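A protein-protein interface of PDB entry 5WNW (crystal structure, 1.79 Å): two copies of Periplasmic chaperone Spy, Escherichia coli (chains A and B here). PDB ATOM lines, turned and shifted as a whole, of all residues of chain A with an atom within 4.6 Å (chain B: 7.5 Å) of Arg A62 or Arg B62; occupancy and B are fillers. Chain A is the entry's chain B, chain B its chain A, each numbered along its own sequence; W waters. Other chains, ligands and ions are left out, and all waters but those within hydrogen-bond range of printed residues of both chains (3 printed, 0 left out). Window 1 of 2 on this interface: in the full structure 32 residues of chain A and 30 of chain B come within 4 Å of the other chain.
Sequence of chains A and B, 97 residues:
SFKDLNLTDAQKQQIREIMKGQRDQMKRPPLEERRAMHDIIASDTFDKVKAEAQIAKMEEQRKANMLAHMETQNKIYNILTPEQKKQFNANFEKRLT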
ATOM      1  N   MET A  58      -7.183 -18.026 -22.365  1.00  0.00           N
ATOM      2  CA  MET A  58      -6.448 -19.279 -22.231  1.00  0.00           C
ATOM      3  C   MET A  58      -5.151 -19.151 -21.399  1.00  0.00           C
ATOM      4  O   MET A  58      -4.774 -20.100 -20.724  1.00  0.00           O
ATOM      5  CB  MET A  58      -6.103 -19.859 -23.601  1.00  0.00           C
ATOM      6  CG  MET A  58      -7.323 -20.364 -24.367  1.00  0.00           C
ATOM      7  SD  MET A  58      -6.946 -20.686 -26.098  1.00  0.00           S
ATOM      8  CE  MET A  58      -8.533 -21.383 -26.628  1.00  0.00           C
ATOM      9  N   GLU A  59      -4.454 -18.019 -21.498  1.00  0.00           N
ATOM     10  CA  GLU A  59      -3.300 -17.736 -20.625  1.00  0.00           C
ATOM     11  C   GLU A  59      -3.615 -17.833 -19.138  1.00  0.00           C
ATOM     12  O   GLU A  59      -2.757 -18.230 -18.328  1.00  0.00           O
ATOM     13  CB  GLU A  59      -2.739 -16.358 -20.941  1.00  0.00           C
ATOM     14  CG  GLU A  59      -2.053 -16.248 -22.286  1.00  0.00           C
ATOM     15  CD  GLU A  59      -0.714 -16.983 -22.363  1.00  0.00           C
ATOM     16  OE1 GLU A  59       0.046 -17.005 -21.355  1.00  0.00           O
ATOM     17  OE2 GLU A  59      -0.413 -17.517 -23.457  1.00  0.00           O
ATOM     18  N   GLU A  60      -4.806 -17.428 -18.716  1.00  0.00           N
ATOM     19  CA  GLU A  60      -5.230 -17.591 -17.328  1.00  0.00           C
ATOM     20  C   GLU A  60      -5.215 -19.042 -16.933  1.00  0.00           C
ATOM     21  O   GLU A  60      -4.713 -19.439 -15.893  1.00  0.00           O
ATOM     22  CB  GLU A  60      -6.649 -17.080 -17.102  1.00  0.00           C
ATOM     23  CG  GLU A  60      -6.842 -15.618 -17.263  1.00  0.00           C
ATOM     24  CD  GLU A  60      -8.138 -15.156 -16.616  1.00  0.00           C
ATOM     25  OE1 GLU A  60      -8.986 -14.610 -17.333  1.00  0.00           O
ATOM     26  OE2 GLU A  60      -8.307 -15.342 -15.388  1.00  0.00           O
ATOM     27  N   GLN A  61      -5.824 -19.862 -17.786  1.00  0.00           N
ATOM     28  CA  GLN A  61      -5.961 -21.256 -17.404  1.00  0.00           C
ATOM     29  C   GLN A  61      -4.623 -21.949 -17.466  1.00  0.00           C
ATOM     30  O   GLN A  61      -4.308 -22.772 -16.614  1.00  0.00           O
ATOM     31  CB  GLN A  61      -6.965 -21.988 -18.288  1.00  0.00           C
ATOM     32  CG  GLN A  61      -7.281 -23.377 -17.756  1.00  0.00           C
ATOM     33  CD  GLN A  61      -7.667 -23.352 -16.293  1.00  0.00           C
ATOM     34  OE1 GLN A  61      -7.220 -24.189 -15.496  1.00  0.00           O
ATOM     35  NE2 GLN A  61      -8.494 -22.368 -15.922  1.00  0.00           N
ATOM     36  N   ARG A  62      -3.835 -21.615 -18.480  1.00  0.00           N
ATOM     37  CA  ARG A  62      -2.475 -22.119 -18.578  1.00  0.00           C
ATOM     38  C   ARG A  62      -1.660 -21.762 -17.353  1.00  0.00           C
ATOM     39  O   ARG A  62      -0.887 -22.588 -16.848  1.00  0.00           O
ATOM     40  CB  ARG A  62      -1.791 -21.567 -19.830  1.00  0.00           C
ATOM     41  CG  ARG A  62      -0.329 -21.969 -19.978  1.00  0.00           C
ATOM     42  CD  ARG A  62       0.181 -21.770 -21.423  1.00  0.00           C
ATOM     43  NE  ARG A  62       1.577 -22.197 -21.503  1.00  0.00           N
ATOM     44  CZ  ARG A  62       2.576 -21.535 -20.926  1.00  0.00           C
ATOM     45  NH1 ARG A  62       2.331 -20.433 -20.234  1.00  0.00           N
ATOM     46  NH2 ARG A  62       3.823 -21.973 -21.022  1.00  0.00           N
ATOM     47  N   LYS A  63      -1.808 -20.545 -16.845  1.00  0.00           N
ATOM     48  CA  LYS A  63      -1.020 -20.153 -15.723  1.00  0.00           C
ATOM     49  C   LYS A  63      -1.344 -21.021 -14.513  1.00  0.00           C
ATOM     50  O   LYS A  63      -0.443 -21.520 -13.796  1.00  0.00           O
ATOM     51  CB  LYS A  63      -1.259 -18.688 -15.390  1.00  0.00           C
ATOM     52  CG  LYS A  63      -0.460 -18.233 -14.212  1.00  0.00           C
ATOM     53  CD  LYS A  63      -0.877 -16.849 -13.808  1.00  0.00           C
ATOM     54  CE  LYS A  63      -0.329 -16.466 -12.461  1.00  0.00           C
ATOM     55  NZ  LYS A  63      -1.011 -15.226 -11.958  1.00  0.00           N
ATOM     56  N   ALA A  64      -2.630 -21.222 -14.274  1.00  0.00           N
ATOM     57  CA  ALA A  64      -3.052 -22.060 -13.157  1.00  0.00           C
ATOM     58  C   ALA A  64      -2.563 -23.510 -13.296  1.00  0.00           C
ATOM     59  O   ALA A  64      -2.118 -24.103 -12.329  1.00  0.00           O
ATOM     60  CB  ALA A  64      -4.559 -22.030 -13.034  1.00  0.00           C
ATOM     61  N   ASN A  65      -2.658 -24.058 -14.501  1.00  0.00           N
ATOM     62  CA  ASN A  65      -2.281 -25.444 -14.751  1.00  0.00           C
ATOM     63  C   ASN A  65      -0.794 -25.650 -14.645  1.00  0.00           C
ATOM     64  O   ASN A  65      -0.356 -26.646 -14.065  1.00  0.00           O
ATOM     65  CB  ASN A  65      -2.778 -25.883 -16.131  1.00  0.00           C
ATOM     66  CG  ASN A  65      -4.270 -26.089 -16.162  1.00  0.00           C
ATOM     67  OD1 ASN A  65      -4.898 -26.293 -15.120  1.00  0.00           O
ATOM     68  ND2 ASN A  65      -4.854 -26.053 -17.360  1.00  0.00           N
ATOM     69  N   MET A  66      -0.004 -24.723 -15.199  1.00  0.00           N
ATOM     70  CA  MET A  66       1.455 -24.822 -15.062  1.00  0.00           C
ATOM     71  C   MET A  66       1.921 -24.651 -13.637  1.00  0.00           C
ATOM     72  O   MET A  66       2.828 -25.358 -13.195  1.00  0.00           O
ATOM     73  CB  MET A  66       2.184 -23.804 -15.928  1.00  0.00           C
ATOM     74  CG  MET A  66       2.113 -24.093 -17.411  1.00  0.00           C
ATOM     75  SD  MET A  66       2.804 -25.681 -17.914  1.00  0.00           S
ATOM     76  CE  MET A  66       4.183 -25.897 -16.821  1.00  0.00           C
ATOM     77  N   GLU B  33      12.894 -22.891 -22.760  1.00  0.00           N
ATOM     78  CA  GLU B  33      11.763 -22.916 -21.843  1.00  0.00           C
ATOM     79  C   GLU B  33      11.782 -24.153 -20.939  1.00  0.00           C
ATOM     80  O   GLU B  33      11.459 -24.058 -19.746  1.00  0.00           O
ATOM     81  CB  GLU B  33      10.448 -22.861 -22.640  1.00  0.00           C
ATOM     82  CG  GLU B  33       9.185 -23.030 -21.778  1.00  0.00           C
ATOM     83  CD  GLU B  33       8.024 -22.136 -22.220  1.00  0.00           C
ATOM     84  OE1 GLU B  33       8.177 -20.899 -22.135  1.00  0.00           O
ATOM     85  OE2 GLU B  33       6.963 -22.660 -22.640  1.00  0.00           O
ATOM     86  N   MET B  37      11.988 -24.387 -16.767  1.00  0.00           N
ATOM     87  CA  MET B  37      11.096 -25.206 -15.955  1.00  0.00           C
ATOM     88  C   MET B  37      11.900 -26.155 -15.095  1.00  0.00           C
ATOM     89  O   MET B  37      11.576 -26.406 -13.935  1.00  0.00           O
ATOM     90  CB  MET B  37      10.142 -26.049 -16.812  1.00  0.00           C
ATOM     91  CG  MET B  37       8.874 -25.400 -17.230  1.00  0.00           C
ATOM     92  SD  MET B  37       7.847 -26.573 -18.164  1.00  0.00           S
ATOM     93  CE  MET B  37       7.463 -27.768 -16.887  1.00  0.00           C
ATOM     94  N   GLU B  52       5.975 -17.923 -11.968  1.00  0.00           N
ATOM     95  CA  GLU B  52       5.029 -17.110 -12.727  1.00  0.00           C
ATOM     96  C   GLU B  52       5.749 -16.344 -13.837  1.00  0.00           C
ATOM     97  O   GLU B  52       5.226 -16.213 -14.926  1.00  0.00           O
ATOM     98  CB  GLU B  52       4.263 -16.151 -11.815  1.00  0.00           C
ATOM     99  CG  GLU B  52       3.205 -16.827 -10.949  1.00  0.00           C
ATOM    100  CD  GLU B  52       2.144 -15.848 -10.437  1.00  0.00           C
ATOM    101  OE1 GLU B  52       2.283 -14.628 -10.659  1.00  0.00           O
ATOM    102  OE2 GLU B  52       1.160 -16.304  -9.823  1.00  0.00           O
ATOM    103  N   ALA B  53       6.960 -15.873 -13.579  1.00  0.00           N
ATOM    104  CA  ALA B  53       7.697 -15.128 -14.587  1.00  0.00           C
ATOM    105  C   ALA B  53       8.031 -16.066 -15.732  1.00  0.00           C
ATOM    106  O   ALA B  53       7.895 -15.714 -16.892  1.00  0.00           O
ATOM    107  CB  ALA B  53       8.962 -14.511 -14.001  1.00  0.00           C
ATOM    108  N   GLN B  54       8.498 -17.257 -15.366  1.00  0.00           N
ATOM    109  CA  GLN B  54       8.770 -18.330 -16.323  1.00  0.00           C
ATOM    110  C   GLN B  54       7.595 -18.603 -17.248  1.00  0.00           C
ATOM    111  O   GLN B  54       7.729 -18.669 -18.469  1.00  0.00           O
ATOM    112  CB  GLN B  54       9.127 -19.615 -15.567  1.00  0.00           C
ATOM    113  CG  GLN B  54       9.741 -20.738 -16.417  1.00  0.00           C
ATOM    114  CD  GLN B  54       8.732 -21.491 -17.284  1.00  0.00           C
ATOM    115  OE1 GLN B  54       8.960 -21.735 -18.487  1.00  0.00           O
ATOM    116  NE2 GLN B  54       7.636 -21.902 -16.675  1.00  0.00           N
ATOM    117  N   ILE B  55       6.423 -18.731 -16.650  1.00  0.00           N
ATOM    118  CA  ILE B  55       5.222 -19.088 -17.379  1.00  0.00           C
ATOM    119  C   ILE B  55       4.878 -17.982 -18.370  1.00  0.00           C
ATOM    120  O   ILE B  55       4.439 -18.249 -19.487  1.00  0.00           O
ATOM    121  CB  ILE B  55       4.062 -19.333 -16.382  1.00  0.00           C
ATOM    122  CG1 ILE B  55       4.314 -20.643 -15.637  1.00  0.00           C
ATOM    123  CG2 ILE B  55       2.717 -19.353 -17.083  1.00  0.00           C
ATOM    124  CD1 ILE B  55       3.475 -20.810 -14.392  1.00  0.00           C
ATOM    125  N   ALA B  56       5.126 -16.734 -17.964  1.00  0.00           N
ATOM    126  CA  ALA B  56       4.738 -15.581 -18.773  1.00  0.00           C
ATOM    127  C   ALA B  56       5.699 -15.251 -19.908  1.00  0.00           C
ATOM    128  O   ALA B  56       5.327 -14.497 -20.821  1.00  0.00           O
ATOM    129  CB  ALA B  56       4.615 -14.371 -17.880  1.00  0.00           C
ATOM    130  N   LYS B  57       6.928 -15.751 -19.819  1.00  0.00           N
ATOM    131  CA  LYS B  57       8.033 -15.253 -20.629  1.00  0.00           C
ATOM    132  C   LYS B  57       7.671 -15.369 -22.103  1.00  0.00           C
ATOM    133  O   LYS B  57       7.856 -14.426 -22.870  1.00  0.00           O
ATOM    134  CB  LYS B  57       9.340 -15.994 -20.336  1.00  0.00           C
ATOM    135  CG  LYS B  57      10.556 -15.253 -20.909  1.00  0.00           C
ATOM    136  CD  LYS B  57      11.762 -16.168 -21.158  1.00  0.00           C
ATOM    137  CE  LYS B  57      12.343 -16.703 -19.862  1.00  0.00           C
ATOM    138  NZ  LYS B  57      13.346 -17.823 -20.038  1.00  0.00           N
ATOM    139  N   MET B  58       7.102 -16.498 -22.490  1.00  0.00           N
ATOM    140  CA  MET B  58       6.855 -16.722 -23.919  1.00  0.00           C
ATOM    141  C   MET B  58       5.431 -16.371 -24.374  1.00  0.00           C
ATOM    142  O   MET B  58       4.939 -16.908 -25.375  1.00  0.00           O
ATOM    143  CB  MET B  58       7.156 -18.178 -24.266  1.00  0.00           C
ATOM    144  CG  MET B  58       8.605 -18.610 -23.962  1.00  0.00           C
ATOM    145  SD  MET B  58       9.872 -17.518 -24.659  1.00  0.00           S
ATOM    146  CE  MET B  58       9.635 -17.700 -26.403  1.00  0.00           C
ATOM    147  N   GLU B  59       4.788 -15.441 -23.680  1.00  0.00           N
ATOM    148  CA  GLU B  59       3.426 -15.051 -24.010  1.00  0.00           C
ATOM    149  C   GLU B  59       3.259 -14.584 -25.456  1.00  0.00           C
ATOM    150  O   GLU B  59       2.287 -14.941 -26.111  1.00  0.00           O
ATOM    151  CB  GLU B  59       2.961 -13.937 -23.063  1.00  0.00           C
ATOM    152  CG  GLU B  59       1.596 -13.382 -23.323  1.00  0.00           C
ATOM    153  CD  GLU B  59       1.338 -12.147 -22.408  1.00  0.00           C
ATOM    154  OE1 GLU B  59       1.762 -12.169 -21.238  1.00  0.00           O
ATOM    155  OE2 GLU B  59       0.729 -11.172 -22.876  1.00  0.00           O
ATOM    156  N   GLU B  60       4.188 -13.772 -25.952  1.00  0.00           N
ATOM    157  CA  GLU B  60       4.049 -13.237 -27.315  1.00  0.00           C
ATOM    158  C   GLU B  60       4.167 -14.325 -28.377  1.00  0.00           C
ATOM    159  O   GLU B  60       3.412 -14.332 -29.364  1.00  0.00           O
ATOM    160  CB  GLU B  60       5.090 -12.154 -27.575  1.00  0.00           C
ATOM    161  N   GLN B  61       5.118 -15.235 -28.191  1.00  0.00           N
ATOM    162  CA  GLN B  61       5.328 -16.296 -29.162  1.00  0.00           C
ATOM    163  C   GLN B  61       4.135 -17.243 -29.151  1.00  0.00           C
ATOM    164  O   GLN B  61       3.694 -17.690 -30.224  1.00  0.00           O
ATOM    165  CB  GLN B  61       6.636 -17.043 -28.868  1.00  0.00           C
ATOM    166  N   ARG B  62       3.580 -17.526 -27.965  1.00  0.00           N
ATOM    167  CA  ARG B  62       2.376 -18.373 -27.871  1.00  0.00           C
ATOM    168  C   ARG B  62       1.189 -17.714 -28.569  1.00  0.00           C
ATOM    169  O   ARG B  62       0.416 -18.377 -29.277  1.00  0.00           O
ATOM    170  CB  ARG B  62       2.004 -18.655 -26.404  1.00  0.00           C
ATOM    171  CG  ARG B  62       2.869 -19.683 -25.704  1.00  0.00           C
ATOM    172  CD  ARG B  62       2.278 -20.150 -24.382  1.00  0.00           C
ATOM    173  NE  ARG B  62       2.095 -19.045 -23.424  1.00  0.00           N
ATOM    174  CZ  ARG B  62       3.017 -18.647 -22.552  1.00  0.00           C
ATOM    175  NH1 ARG B  62       4.219 -19.229 -22.492  1.00  0.00           N
ATOM    176  NH2 ARG B  62       2.726 -17.672 -21.722  1.00  0.00           N
ATOM    177  N   LYS B  63       1.036 -16.408 -28.391  1.00  0.00           N
ATOM    178  CA  LYS B  63      -0.080 -15.709 -29.066  1.00  0.00           C
ATOM    179  C   LYS B  63       0.043 -15.796 -30.592  1.00  0.00           C
ATOM    180  O   LYS B  63      -0.919 -16.134 -31.298  1.00  0.00           O
ATOM    181  CB  LYS B  63      -0.165 -14.258 -28.612  1.00  0.00           C
ATOM    182  CG  LYS B  63      -1.138 -13.349 -29.378  1.00  0.00           C
ATOM    183  CD  LYS B  63      -1.013 -11.865 -28.947  1.00  0.00           C
ATOM    184  CE  LYS B  63      -1.954 -10.983 -29.757  1.00  0.00           C
ATOM    185  NZ  LYS B  63      -1.964  -9.551 -29.195  1.00  0.00           N
ATOM    186  N   ALA B  64       1.236 -15.538 -31.116  1.00  0.00           N
ATOM    187  CA  ALA B  64       1.417 -15.627 -32.566  1.00  0.00           C
ATOM    188  C   ALA B  64       1.149 -17.031 -33.046  1.00  0.00           C
ATOM    189  O   ALA B  64       0.567 -17.230 -34.115  1.00  0.00           O
ATOM    190  CB  ALA B  64       2.799 -15.186 -32.959  1.00  0.00           C
ATOM    191  N   ASN B  65       1.549 -18.025 -32.259  1.00  0.00           N
ATOM    192  CA  ASN B  65       1.398 -19.401 -32.732  1.00  0.00           C
ATOM    193  C   ASN B  65      -0.050 -19.790 -32.730  1.00  0.00           C
ATOM    194  O   ASN B  65      -0.548 -20.357 -33.678  1.00  0.00           O
ATOM    195  CB  ASN B  65       2.196 -20.380 -31.896  1.00  0.00           C
ATOM    196  CG  ASN B  65       3.677 -20.274 -32.155  1.00  0.00           C
ATOM    197  OD1 ASN B  65       4.101 -19.760 -33.201  1.00  0.00           O
ATOM    198  ND2 ASN B  65       4.478 -20.775 -31.219  1.00  0.00           N
ATOM    199  N   MET B  66      -0.743 -19.437 -31.673  1.00  0.00           N
ATOM    200  CA  MET B  66      -2.137 -19.808 -31.557  1.00  0.00           C
ATOM    201  C   MET B  66      -2.995 -19.026 -32.552  1.00  0.00           C
ATOM    202  O   MET B  66      -3.929 -19.568 -33.118  1.00  0.00           O
ATOM    203  CB  MET B  66      -2.630 -19.581 -30.119  1.00  0.00           C
ATOM    204  CG  MET B  66      -4.056 -20.076 -29.917  1.00  0.00           C
ATOM    205  SD  MET B  66      -4.269 -21.856 -30.337  1.00  0.00           S
ATOM    206  CE  MET B  66      -3.225 -22.584 -29.073  1.00  0.00           C
ATOM    207  N   LEU B  67      -2.657 -17.779 -32.837  1.00  0.00           N
ATOM    208  CA  LEU B  67      -3.380 -17.063 -33.883  1.00  0.00           C
ATOM    209  C   LEU B  67      -3.241 -17.707 -35.260  1.00  0.00           C
ATOM    210  O   LEU B  67      -4.223 -17.770 -36.026  1.00  0.00           O
ATOM    211  CB  LEU B  67      -2.910 -15.621 -33.970  1.00  0.00           C
ATOM    212  CG  LEU B  67      -3.473 -14.664 -32.913  1.00  0.00           C
ATOM    213  CD1 LEU B  67      -2.837 -13.287 -33.062  1.00  0.00           C
ATOM    214  CD2 LEU B  67      -4.982 -14.539 -33.041  1.00  0.00           C
ATOM    215  N   ALA B  68      -2.038 -18.185 -35.564  1.00  0.00           N
ATOM    216  CA  ALA B  68      -1.784 -18.904 -36.809  1.00  0.00           C
ATOM    217  C   ALA B  68      -2.621 -20.164 -36.864  1.00  0.00           C
ATOM    218  O   ALA B  68      -3.226 -20.488 -37.893  1.00  0.00           O
ATOM    219  CB  ALA B  68      -0.335 -19.272 -36.917  1.00  0.00           C
HETATM  220  O   HOH W   1       5.224 -23.261 -18.110  1.00  0.00           O
HETATM  221  O   HOH W   2      -0.394 -15.767 -25.561  1.00  0.00           O
HETATM  222  O   HOH W   3       0.993 -14.560 -19.860  1.00  0.00           O
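OE2 of Glu B33 is in salt-bridge range of NH2 of Arg A62 (3.6 Å). OE2 of Glu B52 lies within salt-bridge range of NZ of Lys A63 (3.2 Å). The guanidinium group of Arg A62 sits at hydrogen-bond distance from the backbone carbonyl oxygen of Ile B55 (3.1 Å). NH2 of Arg B62 lies within salt-bridge range of OE1 of Glu A59. The guanidinium group of Arg A62 sits close to the guanidinium group of Arg B62, at 3.1 Å.
O of Ile B55 lies within hydrogen-bond range of NH2 of Arg B62 (2.9 Å).
Among the printed residues, pairs that only touch across the chains: Met A66 with Ile B55 (3.6 Å) and Met A66 with Met B37 (3.8 Å).
Met A58 touches none of the printed residues of chain B. Of the printed residues of chain B, Glu A59 touches Arg B62. Arg A62 touches just these residues of chain B: Glu B33 (3.6 Å), Ile B55 (3.1 Å) and Arg B62 (3.0 Å). Of the printed residues of chain A, Ile B55 touches Arg A62 (3.1 Å) and Met A66 (3.6 Å). Arg B62 touches two residues of chain A. The nearest residue of chain B that does not touch Arg A62 is Ala B56 (5.2 Å).
Hydrophobic or aromatic side chains of chain A that line the printed part of chain B: Met A66. Of the 19 printed residues of chain B, 5 touch a printed residue of chain A. Hydrophobic or aromatic side chains of chain B within 4 Å of the printed part of chain A: Met B37 and Ile B55. Among the printed residues, 7 pairs touch across the chains.
Glu A59 touches Arg B62, but with the chains exchanged Arg A62 does not touch Glu B59 (6.5 Å). Arg B62 touches its own counterpart, Arg A62. 9 positions are printed for both chains. Of the 7 pairs that touch across the chains among the printed residues, 1 has its exchanged pair printed and touching as well.
Water W2 lies within hydrogen-bond range of OE2 of Glu A59 (2.7 Å), O of Glu B59 (2.9 Å) and N of Lys B63 (3.2 Å). Water W3 bridges OE1 of Glu B59 and OE1 of Glu A59. Water W1 lies within hydrogen-bond range of NE2 of Gln B54, SD of Met A66 and NH2 of Arg A62.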
